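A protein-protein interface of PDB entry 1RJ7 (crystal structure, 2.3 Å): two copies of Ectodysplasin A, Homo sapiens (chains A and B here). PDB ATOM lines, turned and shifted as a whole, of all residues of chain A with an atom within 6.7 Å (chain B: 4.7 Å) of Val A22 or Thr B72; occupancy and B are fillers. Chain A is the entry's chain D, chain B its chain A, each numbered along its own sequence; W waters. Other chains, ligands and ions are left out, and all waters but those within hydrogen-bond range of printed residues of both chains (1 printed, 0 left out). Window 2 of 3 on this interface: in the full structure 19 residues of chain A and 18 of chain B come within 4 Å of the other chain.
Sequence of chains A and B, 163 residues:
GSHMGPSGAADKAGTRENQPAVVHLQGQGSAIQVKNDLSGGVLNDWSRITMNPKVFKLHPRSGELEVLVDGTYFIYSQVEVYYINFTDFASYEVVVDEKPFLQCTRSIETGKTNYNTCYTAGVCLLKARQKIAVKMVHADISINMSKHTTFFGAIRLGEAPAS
Printed residues of chain B that touch a printed residue of chain A: Thr B72, Phe B74, Val B123 and Leu B157. Hydrophobic or aromatic side chains of chain B within 4 Å of the printed part of chain A: Phe B74, Val B123 and Leu B157. Along chain B the printed residues that touch a printed residue of chain A span positions 72 to 157. Of the 14 printed residues of chain A, 5 touch a printed residue of chain B. Hydrophobic or aromatic side chains of chain A that line the printed part of chain B: Pro A20, Val A22, His A24 and Ile A155.
Among the printed residues, pairs that only touch across the chains: His A24 with Val B123, Val A22 with Thr B72, Pro A20 with Leu B157, Val A22 with Val B123, Val A23 with Val B123, Ile A155 with Leu B157 and Ile A155 with Phe B74.
Of chain A, only Val A22 (3.7 Å) comes within 4 Å of Thr B72. Printed residues of chain A within 4 Å of Leu B157: Pro A20 (3.7 Å) and Ile A155 (3.8 Å). Printed residues of chain B within 4 Å of Pro A20: Leu B157. Printed residues of chain B within 4 Å of His A24: Val B123 (3.5 Å). Of the printed residues of chain A, Phe B74 touches Ile A155. Of the printed residues of chain A, Val B123 touches Val A22, Val A23 and His A24. Ala A21 touches none of the printed residues of chain B. Met A51 touches none of the printed residues of chain B. The nearest residue of chain B that does not touch Val A22 is Leu B125 (4.2 Å). The nearest residue of chain A that does not touch Thr B72 is Pro A20 (4.4 Å). The nearest printed residue of chain B that does not touch Val A23 is Cys B124 (7.1 Å).
Water W1 lies within hydrogen-bond range of the backbone carbonyl oxygen (O) of Pro A20, the backbone carbonyl oxygen (O) of Glu B159 and the side-chain hydroxyl (OG1) of Thr B72.
2 positions are printed for both chains. Of the 7 pairs that touch across the chains among the printed residues, none has its exchanged pair printed and touching as well.
The backbone carbonyl oxygen of Thr B72 lies within hydrogen-bond range of the backbone NH of Leu B157 (2.8 Å). The backbone NH (N) of Thr B72 sits at hydrogen-bond distance from the backbone carbonyl oxygen (O) of Gly B158 (3.0 Å). The backbone carbonyl oxygen of Phe B74 is in hydrogen-bond range of the backbone NH of Ile B155. N of Asn A52 lies within hydrogen-bond range of O of Val A22 (3.2 Å). O of Ala A154 lies within hydrogen-bond range of N of Val A23, 2.9 Å away. O of Thr A50 sits at hydrogen-bond distance from N of His A24 (3.0 Å).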
ATOM      1  N   PRO A  20       3.846 -22.409   7.233  1.00  0.00           N
ATOM      2  CA  PRO A  20       4.428 -21.716   6.078  1.00  0.00           C
ATOM      3  C   PRO A  20       4.106 -20.221   5.998  1.00  0.00           C
ATOM      4  O   PRO A  20       2.964 -19.817   6.217  1.00  0.00           O
ATOM      5  CB  PRO A  20       3.828 -22.466   4.891  1.00  0.00           C
ATOM      6  CG  PRO A  20       3.613 -23.816   5.412  1.00  0.00           C
ATOM      7  CD  PRO A  20       3.081 -23.595   6.800  1.00  0.00           C
ATOM      8  N   ALA A  21       5.130 -19.428   5.704  1.00  0.00           N
ATOM      9  CA  ALA A  21       4.996 -17.984   5.544  1.00  0.00           C
ATOM     10  C   ALA A  21       5.154 -17.610   4.070  1.00  0.00           C
ATOM     11  O   ALA A  21       5.930 -18.218   3.326  1.00  0.00           O
ATOM     12  CB  ALA A  21       6.017 -17.257   6.401  1.00  0.00           C
ATOM     13  N   VAL A  22       4.407 -16.604   3.648  1.00  0.00           N
ATOM     14  CA  VAL A  22       4.268 -16.300   2.238  1.00  0.00           C
ATOM     15  C   VAL A  22       4.290 -14.812   1.936  1.00  0.00           C
ATOM     16  O   VAL A  22       4.050 -13.991   2.807  1.00  0.00           O
ATOM     17  CB  VAL A  22       2.973 -16.918   1.657  1.00  0.00           C
ATOM     18  CG1 VAL A  22       3.052 -18.421   1.705  1.00  0.00           C
ATOM     19  CG2 VAL A  22       1.733 -16.439   2.402  1.00  0.00           C
ATOM     20  N   VAL A  23       4.570 -14.505   0.670  1.00  0.00           N
ATOM     21  CA  VAL A  23       4.528 -13.161   0.110  1.00  0.00           C
ATOM     22  C   VAL A  23       4.027 -13.211  -1.348  1.00  0.00           C
ATOM     23  O   VAL A  23       4.401 -14.081  -2.118  1.00  0.00           O
ATOM     24  CB  VAL A  23       5.928 -12.477   0.163  1.00  0.00           C
ATOM     25  CG1 VAL A  23       6.991 -13.358  -0.467  1.00  0.00           C
ATOM     26  CG2 VAL A  23       5.901 -11.105  -0.503  1.00  0.00           C
ATOM     27  N   HIS A  24       3.171 -12.271  -1.718  1.00  0.00           N
ATOM     28  CA  HIS A  24       2.747 -12.114  -3.104  1.00  0.00           C
ATOM     29  C   HIS A  24       2.763 -10.652  -3.452  1.00  0.00           C
ATOM     30  O   HIS A  24       1.932  -9.907  -3.000  1.00  0.00           O
ATOM     31  CB  HIS A  24       1.344 -12.689  -3.307  1.00  0.00           C
ATOM     32  CG  HIS A  24       0.891 -12.698  -4.730  1.00  0.00           C
ATOM     33  ND1 HIS A  24       1.328 -13.630  -5.643  1.00  0.00           N
ATOM     34  CD2 HIS A  24       0.015 -11.904  -5.393  1.00  0.00           C
ATOM     35  CE1 HIS A  24       0.770 -13.389  -6.813  1.00  0.00           C
ATOM     36  NE2 HIS A  24      -0.043 -12.355  -6.687  1.00  0.00           N
ATOM     37  N   THR A  50       0.209  -9.165   0.234  1.00  0.00           N
ATOM     38  CA  THR A  50       0.464  -9.959   1.419  1.00  0.00           C
ATOM     39  C   THR A  50       1.981 -10.149   1.566  1.00  0.00           C
ATOM     40  O   THR A  50       2.669 -10.416   0.579  1.00  0.00           O
ATOM     41  CB  THR A  50      -0.321 -11.300   1.327  1.00  0.00           C
ATOM     42  OG1 THR A  50      -0.065 -12.114   2.482  1.00  0.00           O
ATOM     43  CG2 THR A  50       0.120 -12.138   0.134  1.00  0.00           C
ATOM     44  N   MET A  51       2.503  -9.967   2.781  1.00  0.00           N
ATOM     45  CA  MET A  51       3.936 -10.150   3.035  1.00  0.00           C
ATOM     46  C   MET A  51       4.228 -10.348   4.518  1.00  0.00           C
ATOM     47  O   MET A  51       4.109  -9.404   5.316  1.00  0.00           O
ATOM     48  CB  MET A  51       4.748  -8.963   2.504  1.00  0.00           C
ATOM     49  CG  MET A  51       6.268  -9.129   2.628  1.00  0.00           C
ATOM     50  SD  MET A  51       7.200  -7.652   2.068  1.00  0.00           S
ATOM     51  CE  MET A  51       6.787  -6.567   3.346  1.00  0.00           C
ATOM     52  N   ASN A  52       4.622 -11.573   4.875  1.00  0.00           N
ATOM     53  CA  ASN A  52       4.927 -11.912   6.260  1.00  0.00           C
ATOM     54  C   ASN A  52       6.199 -11.164   6.668  1.00  0.00           C
ATOM     55  O   ASN A  52       7.260 -11.476   6.158  1.00  0.00           O
ATOM     56  CB  ASN A  52       5.089 -13.429   6.423  1.00  0.00           C
ATOM     57  CG  ASN A  52       5.084 -13.869   7.885  1.00  0.00           C
ATOM     58  OD1 ASN A  52       5.609 -13.185   8.757  1.00  0.00           O
ATOM     59  ND2 ASN A  52       4.484 -15.020   8.149  1.00  0.00           N
ATOM     60  N   PRO A  53       6.101 -10.165   7.549  1.00  0.00           N
ATOM     61  CA  PRO A  53       7.255  -9.298   7.845  1.00  0.00           C
ATOM     62  C   PRO A  53       8.372  -9.952   8.675  1.00  0.00           C
ATOM     63  O   PRO A  53       9.452  -9.375   8.795  1.00  0.00           O
ATOM     64  CB  PRO A  53       6.628  -8.123   8.634  1.00  0.00           C
ATOM     65  CG  PRO A  53       5.126  -8.295   8.492  1.00  0.00           C
ATOM     66  CD  PRO A  53       4.925  -9.771   8.341  1.00  0.00           C
ATOM     67  N   VAL A  55       9.535 -12.945   7.943  1.00  0.00           N
ATOM     68  CA  VAL A  55      10.288 -13.739   6.981  1.00  0.00           C
ATOM     69  C   VAL A  55      10.726 -12.949   5.731  1.00  0.00           C
ATOM     70  O   VAL A  55      11.782 -13.226   5.175  1.00  0.00           O
ATOM     71  CB  VAL A  55       9.457 -14.971   6.530  1.00  0.00           C
ATOM     72  CG1 VAL A  55      10.182 -15.761   5.415  1.00  0.00           C
ATOM     73  CG2 VAL A  55       9.179 -15.870   7.710  1.00  0.00           C
ATOM     74  N   PHE A  56       9.918 -11.990   5.281  1.00  0.00           N
ATOM     75  CA  PHE A  56      10.195 -11.254   4.036  1.00  0.00           C
ATOM     76  C   PHE A  56      10.238  -9.742   4.206  1.00  0.00           C
ATOM     77  O   PHE A  56       9.440  -9.146   4.937  1.00  0.00           O
ATOM     78  CB  PHE A  56       9.145 -11.558   2.979  1.00  0.00           C
ATOM     79  CG  PHE A  56       9.113 -12.985   2.550  1.00  0.00           C
ATOM     80  CD1 PHE A  56      10.107 -13.506   1.713  1.00  0.00           C
ATOM     81  CD2 PHE A  56       8.080 -13.813   2.960  1.00  0.00           C
ATOM     82  CE1 PHE A  56      10.075 -14.845   1.318  1.00  0.00           C
ATOM     83  CE2 PHE A  56       8.049 -15.146   2.559  1.00  0.00           C
ATOM     84  CZ  PHE A  56       9.053 -15.656   1.739  1.00  0.00           C
ATOM     85  N   ALA A 154       6.671 -15.698  -3.096  1.00  0.00           N
ATOM     86  CA  ALA A 154       7.530 -16.657  -2.409  1.00  0.00           C
ATOM     87  C   ALA A 154       6.841 -17.349  -1.227  1.00  0.00           C
ATOM     88  O   ALA A 154       6.010 -16.752  -0.530  1.00  0.00           O
ATOM     89  CB  ALA A 154       8.813 -15.980  -1.953  1.00  0.00           C
ATOM     90  N   ILE A 155       7.181 -18.625  -1.034  1.00  0.00           N
ATOM     91  CA  ILE A 155       6.656 -19.438   0.046  1.00  0.00           C
ATOM     92  C   ILE A 155       7.822 -20.052   0.791  1.00  0.00           C
ATOM     93  O   ILE A 155       8.584 -20.846   0.234  1.00  0.00           O
ATOM     94  CB  ILE A 155       5.774 -20.580  -0.468  1.00  0.00           C
ATOM     95  CG1 ILE A 155       4.675 -20.067  -1.403  1.00  0.00           C
ATOM     96  CG2 ILE A 155       5.175 -21.372   0.738  1.00  0.00           C
ATOM     97  CD1 ILE A 155       3.958 -21.172  -2.193  1.00  0.00           C
ATOM     98  N   ARG A 156       7.953 -19.700   2.061  1.00  0.00           N
ATOM     99  CA  ARG A 156       8.828 -20.445   2.958  1.00  0.00           C
ATOM    100  C   ARG A 156       8.089 -21.716   3.341  1.00  0.00           C
ATOM    101  O   ARG A 156       7.170 -21.695   4.155  1.00  0.00           O
ATOM    102  CB  ARG A 156       9.210 -19.628   4.186  1.00  0.00           C
ATOM    103  CG  ARG A 156      10.281 -20.296   5.006  1.00  0.00           C
ATOM    104  CD  ARG A 156      10.798 -19.443   6.148  1.00  0.00           C
ATOM    105  NE  ARG A 156      11.890 -20.112   6.833  1.00  0.00           N
ATOM    106  CZ  ARG A 156      11.749 -21.072   7.741  1.00  0.00           C
ATOM    107  NH1 ARG A 156      10.545 -21.505   8.101  1.00  0.00           N
ATOM    108  NH2 ARG A 156      12.826 -21.618   8.287  1.00  0.00           N
ATOM    109  N   GLY B  71      -7.078 -20.400   5.506  1.00  0.00           N
ATOM    110  CA  GLY B  71      -5.705 -20.810   5.320  1.00  0.00           C
ATOM    111  C   GLY B  71      -4.858 -20.053   4.309  1.00  0.00           C
ATOM    112  O   GLY B  71      -5.287 -19.088   3.676  1.00  0.00           O
ATOM    113  N   THR B  72      -3.616 -20.505   4.204  1.00  0.00           N
ATOM    114  CA  THR B  72      -2.695 -20.106   3.155  1.00  0.00           C
ATOM    115  C   THR B  72      -2.798 -21.145   2.055  1.00  0.00           C
ATOM    116  O   THR B  72      -2.607 -22.350   2.298  1.00  0.00           O
ATOM    117  CB  THR B  72      -1.269 -20.067   3.703  1.00  0.00           C
ATOM    118  OG1 THR B  72      -1.221 -19.190   4.844  1.00  0.00           O
ATOM    119  CG2 THR B  72      -0.323 -19.469   2.711  1.00  0.00           C
ATOM    120  N   TYR B  73      -3.109 -20.658   0.858  1.00  0.00           N
ATOM    121  CA  TYR B  73      -3.398 -21.472  -0.308  1.00  0.00           C
ATOM    122  C   TYR B  73      -2.514 -21.029  -1.482  1.00  0.00           C
ATOM    123  O   TYR B  73      -2.351 -19.837  -1.727  1.00  0.00           O
ATOM    124  CB  TYR B  73      -4.882 -21.324  -0.711  1.00  0.00           C
ATOM    125  CG  TYR B  73      -5.872 -21.988   0.225  1.00  0.00           C
ATOM    126  CD1 TYR B  73      -6.368 -21.316   1.352  1.00  0.00           C
ATOM    127  CD2 TYR B  73      -6.326 -23.280  -0.020  1.00  0.00           C
ATOM    128  CE1 TYR B  73      -7.270 -21.918   2.196  1.00  0.00           C
ATOM    129  CE2 TYR B  73      -7.231 -23.887   0.816  1.00  0.00           C
ATOM    130  CZ  TYR B  73      -7.696 -23.211   1.926  1.00  0.00           C
ATOM    131  OH  TYR B  73      -8.593 -23.822   2.773  1.00  0.00           O
ATOM    132  N   PHE B  74      -1.904 -22.004  -2.151  1.00  0.00           N
ATOM    133  CA  PHE B  74      -1.254 -21.824  -3.435  1.00  0.00           C
ATOM    134  C   PHE B  74      -2.267 -22.279  -4.466  1.00  0.00           C
ATOM    135  O   PHE B  74      -2.814 -23.353  -4.362  1.00  0.00           O
ATOM    136  CB  PHE B  74       0.016 -22.681  -3.509  1.00  0.00           C
ATOM    137  CG  PHE B  74       0.782 -22.535  -4.798  1.00  0.00           C
ATOM    138  CD1 PHE B  74       1.333 -21.305  -5.164  1.00  0.00           C
ATOM    139  CD2 PHE B  74       0.968 -23.626  -5.645  1.00  0.00           C
ATOM    140  CE1 PHE B  74       2.047 -21.169  -6.346  1.00  0.00           C
ATOM    141  CE2 PHE B  74       1.667 -23.477  -6.842  1.00  0.00           C
ATOM    142  CZ  PHE B  74       2.212 -22.264  -7.184  1.00  0.00           C
ATOM    143  N   VAL B 123       0.039 -17.298  -4.568  1.00  0.00           N
ATOM    144  CA  VAL B 123      -0.322 -17.608  -3.194  1.00  0.00           C
ATOM    145  C   VAL B 123      -1.172 -16.486  -2.615  1.00  0.00           C
ATOM    146  O   VAL B 123      -0.988 -15.322  -2.947  1.00  0.00           O
ATOM    147  CB  VAL B 123       0.945 -17.898  -2.318  1.00  0.00           C
ATOM    148  CG1 VAL B 123       1.664 -16.631  -1.912  1.00  0.00           C
ATOM    149  CG2 VAL B 123       0.595 -18.699  -1.098  1.00  0.00           C
ATOM    150  N   CYS B 124      -2.127 -16.857  -1.774  1.00  0.00           N
ATOM    151  CA  CYS B 124      -2.982 -15.895  -1.073  1.00  0.00           C
ATOM    152  C   CYS B 124      -3.523 -16.490   0.219  1.00  0.00           C
ATOM    153  O   CYS B 124      -3.395 -17.691   0.469  1.00  0.00           O
ATOM    154  CB  CYS B 124      -4.182 -15.515  -1.942  1.00  0.00           C
ATOM    155  SG  CYS B 124      -5.146 -16.978  -2.394  1.00  0.00           S
ATOM    156  N   LEU B 125      -4.144 -15.638   1.028  1.00  0.00           N
ATOM    157  CA  LEU B 125      -4.860 -16.077   2.224  1.00  0.00           C
ATOM    158  C   LEU B 125      -6.342 -16.098   1.884  1.00  0.00           C
ATOM    159  O   LEU B 125      -6.835 -15.164   1.244  1.00  0.00           O
ATOM    160  CB  LEU B 125      -4.603 -15.127   3.398  1.00  0.00           C
ATOM    161  CG  LEU B 125      -3.153 -14.657   3.594  1.00  0.00           C
ATOM    162  CD1 LEU B 125      -3.057 -13.665   4.738  1.00  0.00           C
ATOM    163  CD2 LEU B 125      -2.178 -15.821   3.820  1.00  0.00           C
ATOM    164  N   ILE B 155      -3.363 -25.956  -3.097  1.00  0.00           N
ATOM    165  CA  ILE B 155      -2.721 -26.579  -1.950  1.00  0.00           C
ATOM    166  C   ILE B 155      -3.051 -25.727  -0.742  1.00  0.00           C
ATOM    167  O   ILE B 155      -2.726 -24.539  -0.720  1.00  0.00           O
ATOM    168  CB  ILE B 155      -1.164 -26.623  -2.103  1.00  0.00           C
ATOM    169  CG1 ILE B 155      -0.726 -27.349  -3.370  1.00  0.00           C
ATOM    170  CG2 ILE B 155      -0.518 -27.277  -0.868  1.00  0.00           C
ATOM    171  CD1 ILE B 155       0.769 -27.124  -3.712  1.00  0.00           C
ATOM    172  N   ARG B 156      -3.691 -26.305   0.262  1.00  0.00           N
ATOM    173  CA  ARG B 156      -3.712 -25.661   1.567  1.00  0.00           C
ATOM    174  C   ARG B 156      -2.371 -25.910   2.258  1.00  0.00           C
ATOM    175  O   ARG B 156      -2.139 -26.968   2.821  1.00  0.00           O
ATOM    176  CB  ARG B 156      -4.853 -26.143   2.437  1.00  0.00           C
ATOM    177  CG  ARG B 156      -4.973 -25.320   3.710  1.00  0.00           C
ATOM    178  CD  ARG B 156      -6.196 -25.651   4.534  1.00  0.00           C
ATOM    179  NE  ARG B 156      -6.289 -24.819   5.724  1.00  0.00           N
ATOM    180  CZ  ARG B 156      -5.583 -24.991   6.836  1.00  0.00           C
ATOM    181  NH1 ARG B 156      -4.685 -25.960   6.943  1.00  0.00           N
ATOM    182  NH2 ARG B 156      -5.768 -24.175   7.860  1.00  0.00           N
ATOM    183  N   LEU B 157      -1.493 -24.917   2.182  1.00  0.00           N
ATOM    184  CA  LEU B 157      -0.151 -25.006   2.738  1.00  0.00           C
ATOM    185  C   LEU B 157      -0.151 -25.159   4.249  1.00  0.00           C
ATOM    186  O   LEU B 157       0.652 -25.913   4.804  1.00  0.00           O
ATOM    187  CB  LEU B 157       0.643 -23.756   2.348  1.00  0.00           C
ATOM    188  CG  LEU B 157       0.907 -23.655   0.843  1.00  0.00           C
ATOM    189  CD1 LEU B 157       1.474 -22.289   0.495  1.00  0.00           C
ATOM    190  CD2 LEU B 157       1.857 -24.748   0.393  1.00  0.00           C
ATOM    191  N   GLY B 158      -1.055 -24.421   4.889  1.00  0.00           N
ATOM    192  CA  GLY B 158      -1.234 -24.423   6.331  1.00  0.00           C
ATOM    193  C   GLY B 158      -2.204 -23.336   6.776  1.00  0.00           C
ATOM    194  O   GLY B 158      -3.024 -22.851   5.990  1.00  0.00           O
ATOM    195  N   GLU B 159      -2.117 -22.940   8.038  1.00  0.00           N
ATOM    196  CA  GLU B 159      -2.975 -21.881   8.564  1.00  0.00           C
ATOM    197  C   GLU B 159      -2.611 -20.521   7.954  1.00  0.00           C
ATOM    198  O   GLU B 159      -1.495 -20.325   7.423  1.00  0.00           O
ATOM    199  CB  GLU B 159      -2.886 -21.813  10.095  1.00  0.00           C
ATOM    200  CG  GLU B 159      -3.352 -23.082  10.819  1.00  0.00           C
ATOM    201  CD  GLU B 159      -4.871 -23.209  10.948  1.00  0.00           C
ATOM    202  OE1 GLU B 159      -5.587 -22.182  10.997  1.00  0.00           O
ATOM    203  OE2 GLU B 159      -5.360 -24.357  11.012  1.00  0.00           O
ATOM    204  N   ALA B 160      -3.577 -19.608   7.996  1.00  0.00           N
ATOM    205  CA  ALA B 160      -3.345 -18.201   7.693  1.00  0.00           C
ATOM    206  C   ALA B 160      -2.905 -17.484   8.968  1.00  0.00           C
ATOM    207  O   ALA B 160      -3.426 -17.790  10.041  1.00  0.00           O
ATOM    208  CB  ALA B 160      -4.623 -17.563   7.153  1.00  0.00           C
ATOM    209  N   PRO B 161      -1.975 -16.527   8.871  1.00  0.00           N
ATOM    210  CA  PRO B 161      -1.583 -15.702  10.025  1.00  0.00           C
ATOM    211  C   PRO B 161      -2.794 -15.108  10.755  1.00  0.00           C
ATOM    212  O   PRO B 161      -3.721 -14.658  10.082  1.00  0.00           O
ATOM    213  CB  PRO B 161      -0.752 -14.587   9.380  1.00  0.00           C
ATOM    214  CG  PRO B 161      -0.186 -15.195   8.156  1.00  0.00           C
ATOM    215  CD  PRO B 161      -1.232 -16.137   7.660  1.00  0.00           C
HETATM  216  O   HOH W   1       0.922 -21.643   5.870  1.00  0.00           O
